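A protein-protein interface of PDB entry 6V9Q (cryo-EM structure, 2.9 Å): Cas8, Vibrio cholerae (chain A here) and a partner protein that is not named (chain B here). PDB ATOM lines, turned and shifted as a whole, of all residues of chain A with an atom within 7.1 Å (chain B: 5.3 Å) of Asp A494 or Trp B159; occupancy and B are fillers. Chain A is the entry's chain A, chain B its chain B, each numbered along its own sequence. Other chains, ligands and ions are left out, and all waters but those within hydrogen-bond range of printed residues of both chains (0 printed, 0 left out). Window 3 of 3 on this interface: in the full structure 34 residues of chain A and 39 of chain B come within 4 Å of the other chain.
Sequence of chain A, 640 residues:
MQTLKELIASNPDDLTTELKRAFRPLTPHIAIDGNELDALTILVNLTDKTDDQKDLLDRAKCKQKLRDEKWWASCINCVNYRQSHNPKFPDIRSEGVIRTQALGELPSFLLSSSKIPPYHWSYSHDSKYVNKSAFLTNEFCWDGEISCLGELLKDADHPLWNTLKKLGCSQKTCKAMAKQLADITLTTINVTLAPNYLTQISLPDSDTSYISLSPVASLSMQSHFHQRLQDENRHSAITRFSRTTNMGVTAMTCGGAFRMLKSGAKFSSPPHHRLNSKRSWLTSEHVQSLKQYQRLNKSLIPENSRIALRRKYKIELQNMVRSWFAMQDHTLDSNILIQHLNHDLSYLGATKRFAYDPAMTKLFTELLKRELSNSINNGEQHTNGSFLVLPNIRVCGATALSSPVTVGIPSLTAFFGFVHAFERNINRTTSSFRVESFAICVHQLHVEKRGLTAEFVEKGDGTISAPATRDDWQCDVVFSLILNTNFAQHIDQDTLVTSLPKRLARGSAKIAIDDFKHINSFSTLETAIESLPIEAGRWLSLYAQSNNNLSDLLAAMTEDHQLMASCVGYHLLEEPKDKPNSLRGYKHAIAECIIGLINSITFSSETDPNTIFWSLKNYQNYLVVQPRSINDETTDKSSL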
ATOM      1  N   ILE A 491     -17.611  -9.946  24.140  1.00  0.00           N
ATOM      2  CA  ILE A 491     -16.204 -10.197  24.417  1.00  0.00           C
ATOM      3  C   ILE A 491     -15.887 -11.626  23.999  1.00  0.00           C
ATOM      4  O   ILE A 491     -16.673 -12.537  24.263  1.00  0.00           O
ATOM      5  CB  ILE A 491     -15.882  -9.944  25.898  1.00  0.00           C
ATOM      6  CG1 ILE A 491     -16.269  -8.522  26.279  1.00  0.00           C
ATOM      7  CG2 ILE A 491     -14.402 -10.112  26.178  1.00  0.00           C
ATOM      8  CD1 ILE A 491     -16.221  -8.281  27.752  1.00  0.00           C
ATOM      9  N   ASP A 492     -14.749 -11.809  23.328  1.00  0.00           N
ATOM     10  CA  ASP A 492     -14.366 -13.121  22.821  1.00  0.00           C
ATOM     11  C   ASP A 492     -14.066 -14.083  23.962  1.00  0.00           C
ATOM     12  O   ASP A 492     -13.734 -13.669  25.075  1.00  0.00           O
ATOM     13  CB  ASP A 492     -13.142 -13.004  21.914  1.00  0.00           C
ATOM     14  CG  ASP A 492     -13.453 -12.320  20.604  1.00  0.00           C
ATOM     15  OD1 ASP A 492     -14.605 -12.430  20.137  1.00  0.00           O
ATOM     16  OD2 ASP A 492     -12.547 -11.674  20.039  1.00  0.00           O
ATOM     17  N   GLN A 493     -14.208 -15.379  23.675  1.00  0.00           N
ATOM     18  CA  GLN A 493     -13.852 -16.405  24.648  1.00  0.00           C
ATOM     19  C   GLN A 493     -12.357 -16.398  24.926  1.00  0.00           C
ATOM     20  O   GLN A 493     -11.932 -16.591  26.067  1.00  0.00           O
ATOM     21  CB  GLN A 493     -14.295 -17.777  24.146  1.00  0.00           C
ATOM     22  CG  GLN A 493     -14.047 -18.920  25.113  1.00  0.00           C
ATOM     23  CD  GLN A 493     -14.481 -20.261  24.555  1.00  0.00           C
ATOM     24  OE1 GLN A 493     -14.965 -20.350  23.429  1.00  0.00           O
ATOM     25  NE2 GLN A 493     -14.293 -21.313  25.334  1.00  0.00           N
ATOM     26  N   ASP A 494     -11.545 -16.146  23.898  1.00  0.00           N
ATOM     27  CA  ASP A 494     -10.098 -16.121  24.081  1.00  0.00           C
ATOM     28  C   ASP A 494      -9.666 -14.916  24.902  1.00  0.00           C
ATOM     29  O   ASP A 494      -8.618 -14.942  25.552  1.00  0.00           O
ATOM     30  CB  ASP A 494      -9.402 -16.113  22.725  1.00  0.00           C
ATOM     31  CG  ASP A 494      -9.668 -17.369  21.932  1.00  0.00           C
ATOM     32  OD1 ASP A 494      -9.921 -18.421  22.553  1.00  0.00           O
ATOM     33  OD2 ASP A 494      -9.626 -17.304  20.686  1.00  0.00           O
ATOM     34  N   THR A 495     -10.458 -13.846  24.884  1.00  0.00           N
ATOM     35  CA  THR A 495     -10.126 -12.679  25.688  1.00  0.00           C
ATOM     36  C   THR A 495     -10.554 -12.883  27.135  1.00  0.00           C
ATOM     37  O   THR A 495      -9.851 -12.474  28.064  1.00  0.00           O
ATOM     38  CB  THR A 495     -10.777 -11.432  25.085  1.00  0.00           C
ATOM     39  OG1 THR A 495     -10.375 -11.311  23.717  1.00  0.00           O
ATOM     40  CG2 THR A 495     -10.339 -10.175  25.820  1.00  0.00           C
ATOM     41  N   LEU A 496     -11.695 -13.541  27.348  1.00  0.00           N
ATOM     42  CA  LEU A 496     -12.189 -13.744  28.707  1.00  0.00           C
ATOM     43  C   LEU A 496     -11.333 -14.740  29.473  1.00  0.00           C
ATOM     44  O   LEU A 496     -11.200 -14.641  30.695  1.00  0.00           O
ATOM     45  CB  LEU A 496     -13.643 -14.210  28.695  1.00  0.00           C
ATOM     46  CG  LEU A 496     -14.733 -13.195  28.383  1.00  0.00           C
ATOM     47  CD1 LEU A 496     -16.076 -13.892  28.357  1.00  0.00           C
ATOM     48  CD2 LEU A 496     -14.728 -12.102  29.420  1.00  0.00           C
ATOM     49  N   VAL A 497     -10.746 -15.712  28.778  1.00  0.00           N
ATOM     50  CA  VAL A 497      -9.964 -16.734  29.468  1.00  0.00           C
ATOM     51  C   VAL A 497      -8.588 -16.194  29.841  1.00  0.00           C
ATOM     52  O   VAL A 497      -8.133 -16.342  30.981  1.00  0.00           O
ATOM     53  CB  VAL A 497      -9.869 -18.005  28.609  1.00  0.00           C
ATOM     54  CG1 VAL A 497      -8.894 -18.980  29.214  1.00  0.00           C
ATOM     55  CG2 VAL A 497     -11.228 -18.652  28.512  1.00  0.00           C
ATOM     56  N   THR A 498      -7.918 -15.530  28.899  1.00  0.00           N
ATOM     57  CA  THR A 498      -6.552 -15.084  29.156  1.00  0.00           C
ATOM     58  C   THR A 498      -6.507 -13.859  30.059  1.00  0.00           C
ATOM     59  O   THR A 498      -5.434 -13.496  30.549  1.00  0.00           O
ATOM     60  CB  THR A 498      -5.835 -14.792  27.844  1.00  0.00           C
ATOM     61  OG1 THR A 498      -6.497 -13.720  27.165  1.00  0.00           O
ATOM     62  CG2 THR A 498      -5.847 -16.014  26.960  1.00  0.00           C
ATOM     63  N   SER A 499      -7.645 -13.206  30.284  1.00  0.00           N
ATOM     64  CA  SER A 499      -7.674 -12.080  31.204  1.00  0.00           C
ATOM     65  C   SER A 499      -8.078 -12.493  32.608  1.00  0.00           C
ATOM     66  O   SER A 499      -8.193 -11.627  33.479  1.00  0.00           O
ATOM     67  CB  SER A 499      -8.625 -11.004  30.691  1.00  0.00           C
ATOM     68  OG  SER A 499      -9.956 -11.481  30.672  1.00  0.00           O
ATOM     69  N   ILE A 513     -11.601 -26.596  31.462  1.00  0.00           N
ATOM     70  CA  ILE A 513     -11.840 -26.338  30.046  1.00  0.00           C
ATOM     71  C   ILE A 513     -13.277 -26.691  29.674  1.00  0.00           C
ATOM     72  O   ILE A 513     -13.916 -26.004  28.867  1.00  0.00           O
ATOM     73  CB  ILE A 513     -10.809 -27.105  29.197  1.00  0.00           C
ATOM     74  CG1 ILE A 513      -9.409 -26.585  29.494  1.00  0.00           C
ATOM     75  CG2 ILE A 513     -11.082 -26.985  27.712  1.00  0.00           C
ATOM     76  CD1 ILE A 513      -8.341 -27.390  28.843  1.00  0.00           C
ATOM     77  N   PHE A 516     -15.540 -23.785  30.176  1.00  0.00           N
ATOM     78  CA  PHE A 516     -15.386 -22.588  29.358  1.00  0.00           C
ATOM     79  C   PHE A 516     -16.634 -22.281  28.544  1.00  0.00           C
ATOM     80  O   PHE A 516     -16.751 -21.176  28.004  1.00  0.00           O
ATOM     81  CB  PHE A 516     -14.189 -22.714  28.416  1.00  0.00           C
ATOM     82  CG  PHE A 516     -12.857 -22.504  29.080  1.00  0.00           C
ATOM     83  CD1 PHE A 516     -12.769 -21.942  30.340  1.00  0.00           C
ATOM     84  CD2 PHE A 516     -11.687 -22.847  28.422  1.00  0.00           C
ATOM     85  CE1 PHE A 516     -11.542 -21.742  30.939  1.00  0.00           C
ATOM     86  CE2 PHE A 516     -10.458 -22.649  29.017  1.00  0.00           C
ATOM     87  CZ  PHE A 516     -10.387 -22.097  30.275  1.00  0.00           C
ATOM     88  N   THR B 157      -4.513 -32.863  28.013  1.00  0.00           N
ATOM     89  CA  THR B 157      -5.645 -32.189  27.373  1.00  0.00           C
ATOM     90  C   THR B 157      -5.330 -30.701  27.322  1.00  0.00           C
ATOM     91  O   THR B 157      -5.673 -29.944  28.238  1.00  0.00           O
ATOM     92  CB  THR B 157      -6.956 -32.445  28.116  1.00  0.00           C
ATOM     93  OG1 THR B 157      -7.180 -33.853  28.217  1.00  0.00           O
ATOM     94  CG2 THR B 157      -8.134 -31.829  27.381  1.00  0.00           C
ATOM     95  N   PRO B 158      -4.640 -30.249  26.279  1.00  0.00           N
ATOM     96  CA  PRO B 158      -4.284 -28.831  26.193  1.00  0.00           C
ATOM     97  C   PRO B 158      -5.430 -27.982  25.668  1.00  0.00           C
ATOM     98  O   PRO B 158      -6.322 -28.464  24.972  1.00  0.00           O
ATOM     99  CB  PRO B 158      -3.095 -28.832  25.228  1.00  0.00           C
ATOM    100  CG  PRO B 158      -3.285 -30.027  24.421  1.00  0.00           C
ATOM    101  CD  PRO B 158      -3.935 -31.050  25.266  1.00  0.00           C
ATOM    102  N   TRP B 159      -5.431 -26.702  26.059  1.00  0.00           N
ATOM    103  CA  TRP B 159      -6.559 -25.865  25.651  1.00  0.00           C
ATOM    104  C   TRP B 159      -6.433 -25.214  24.272  1.00  0.00           C
ATOM    105  O   TRP B 159      -7.392 -25.311  23.492  1.00  0.00           O
ATOM    106  CB  TRP B 159      -6.871 -24.785  26.682  1.00  0.00           C
ATOM    107  CG  TRP B 159      -7.985 -23.914  26.217  1.00  0.00           C
ATOM    108  CD1 TRP B 159      -9.259 -24.295  25.937  1.00  0.00           C
ATOM    109  CD2 TRP B 159      -7.922 -22.512  25.971  1.00  0.00           C
ATOM    110  NE1 TRP B 159      -9.999 -23.213  25.535  1.00  0.00           N
ATOM    111  CE2 TRP B 159      -9.196 -22.104  25.550  1.00  0.00           C
ATOM    112  CE3 TRP B 159      -6.912 -21.563  26.069  1.00  0.00           C
ATOM    113  CZ2 TRP B 159      -9.486 -20.785  25.232  1.00  0.00           C
ATOM    114  CZ3 TRP B 159      -7.197 -20.259  25.761  1.00  0.00           C
ATOM    115  CH2 TRP B 159      -8.472 -19.877  25.344  1.00  0.00           C
ATOM    116  N   PRO B 160      -5.310 -24.531  23.894  1.00  0.00           N
ATOM    117  CA  PRO B 160      -5.364 -23.996  22.510  1.00  0.00           C
ATOM    118  C   PRO B 160      -5.036 -25.067  21.476  1.00  0.00           C
ATOM    119  O   PRO B 160      -4.016 -25.040  20.781  1.00  0.00           O
ATOM    120  CB  PRO B 160      -4.332 -22.865  22.553  1.00  0.00           C
ATOM    121  CG  PRO B 160      -3.352 -23.306  23.546  1.00  0.00           C
ATOM    122  CD  PRO B 160      -4.099 -24.059  24.598  1.00  0.00           C
ATOM    123  N   TRP B 161      -5.957 -26.016  21.333  1.00  0.00           N
ATOM    124  CA  TRP B 161      -5.689 -27.310  20.730  1.00  0.00           C
ATOM    125  C   TRP B 161      -6.883 -27.718  19.884  1.00  0.00           C
ATOM    126  O   TRP B 161      -8.022 -27.353  20.181  1.00  0.00           O
ATOM    127  CB  TRP B 161      -5.416 -28.346  21.818  1.00  0.00           C
ATOM    128  CG  TRP B 161      -5.067 -29.722  21.368  1.00  0.00           C
ATOM    129  CD1 TRP B 161      -5.893 -30.799  21.345  1.00  0.00           C
ATOM    130  CD2 TRP B 161      -3.789 -30.186  20.934  1.00  0.00           C
ATOM    131  NE1 TRP B 161      -5.214 -31.903  20.904  1.00  0.00           N
ATOM    132  CE2 TRP B 161      -3.919 -31.551  20.645  1.00  0.00           C
ATOM    133  CE3 TRP B 161      -2.549 -29.579  20.751  1.00  0.00           C
ATOM    134  CZ2 TRP B 161      -2.859 -32.316  20.182  1.00  0.00           C
ATOM    135  CZ3 TRP B 161      -1.500 -30.337  20.297  1.00  0.00           C
ATOM    136  CH2 TRP B 161      -1.660 -31.689  20.013  1.00  0.00           C
ATOM    137  N   MET B 193       3.809 -24.905  22.261  1.00  0.00           N
ATOM    138  CA  MET B 193       2.854 -24.100  23.017  1.00  0.00           C
ATOM    139  C   MET B 193       3.537 -23.339  24.134  1.00  0.00           C
ATOM    140  O   MET B 193       3.228 -22.167  24.374  1.00  0.00           O
ATOM    141  CB  MET B 193       1.758 -24.955  23.629  1.00  0.00           C
ATOM    142  CG  MET B 193       0.694 -25.418  22.714  1.00  0.00           C
ATOM    143  SD  MET B 193      -0.523 -26.203  23.765  1.00  0.00           S
ATOM    144  CE  MET B 193      -1.729 -26.662  22.549  1.00  0.00           C
ATOM    145  N   LEU B 204      -1.076 -18.233  27.348  1.00  0.00           N
ATOM    146  CA  LEU B 204      -1.874 -18.848  28.399  1.00  0.00           C
ATOM    147  C   LEU B 204      -1.564 -20.326  28.620  1.00  0.00           C
ATOM    148  O   LEU B 204      -1.129 -20.674  29.722  1.00  0.00           O
ATOM    149  CB  LEU B 204      -3.343 -18.573  28.065  1.00  0.00           C
ATOM    150  CG  LEU B 204      -4.527 -18.825  28.992  1.00  0.00           C
ATOM    151  CD1 LEU B 204      -5.067 -20.162  28.728  1.00  0.00           C
ATOM    152  CD2 LEU B 204      -4.124 -18.711  30.437  1.00  0.00           C
ATOM    153  N   ILE B 206      -3.013 -23.727  28.864  1.00  0.00           N
ATOM    154  CA  ILE B 206      -3.533 -24.633  29.886  1.00  0.00           C
ATOM    155  C   ILE B 206      -3.278 -26.076  29.471  1.00  0.00           C
ATOM    156  O   ILE B 206      -3.512 -26.447  28.318  1.00  0.00           O
ATOM    157  CB  ILE B 206      -5.034 -24.385  30.122  1.00  0.00           C
ATOM    158  CG1 ILE B 206      -5.268 -23.056  30.808  1.00  0.00           C
ATOM    159  CG2 ILE B 206      -5.665 -25.453  30.985  1.00  0.00           C
ATOM    160  CD1 ILE B 206      -6.720 -22.682  30.867  1.00  0.00           C
ATOM    161  N   PHE B 207      -2.788 -26.890  30.403  1.00  0.00           N
ATOM    162  CA  PHE B 207      -2.760 -28.339  30.274  1.00  0.00           C
ATOM    163  C   PHE B 207      -3.675 -28.958  31.322  1.00  0.00           C
ATOM    164  O   PHE B 207      -3.788 -28.446  32.432  1.00  0.00           O
ATOM    165  CB  PHE B 207      -1.346 -28.874  30.462  1.00  0.00           C
ATOM    166  CG  PHE B 207      -0.413 -28.515  29.358  1.00  0.00           C
ATOM    167  CD1 PHE B 207      -0.883 -28.269  28.087  1.00  0.00           C
ATOM    168  CD2 PHE B 207       0.934 -28.365  29.607  1.00  0.00           C
ATOM    169  CE1 PHE B 207      -0.020 -27.923  27.076  1.00  0.00           C
ATOM    170  CE2 PHE B 207       1.800 -28.012  28.596  1.00  0.00           C
ATOM    171  CZ  PHE B 207       1.319 -27.789  27.335  1.00  0.00           C
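Among the printed residues, pairs that only touch across the chains: Asp A494 with Trp B159, Val A497 with Trp B159, Thr A498 with Leu B204, Ile A513 with Thr B157, Ile A513 with Trp B159, Ile A513 with Ile B206, Phe A516 with Trp B159 and Phe A516 with Ile B206.
The backbone carbonyl oxygen (O) of Ile B206 lies within hydrogen-bond range of the backbone NH (N) of Trp B159 (3.0 Å).
The backbone carbonyl oxygen (O) of Asp A494 lies within hydrogen-bond range of the side-chain hydroxyl (OG1) of Thr A498 (2.9 Å).
Of the printed residues of chain A, Trp B159 touches Asp A494, Val A497, Ile A513 and Phe A516.
Of the printed residues of chain A, Ile B206 touches Ile A513 and Phe A516.
Printed residues of chain A within 4 Å of Thr B157: Ile A513 (3.7 Å).
Printed residues of chain B within 4 Å of Phe A516: Trp B159 and Ile B206.
Of the 9 printed residues of chain B, 4 touch a printed residue of chain A.
Along chain A the printed residues that touch a printed residue of chain B span positions 494 to 516.
Among the printed residues, no Asp or Glu carboxylate lies within 4 Å of a Lys or Arg side-chain nitrogen of the other chain.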
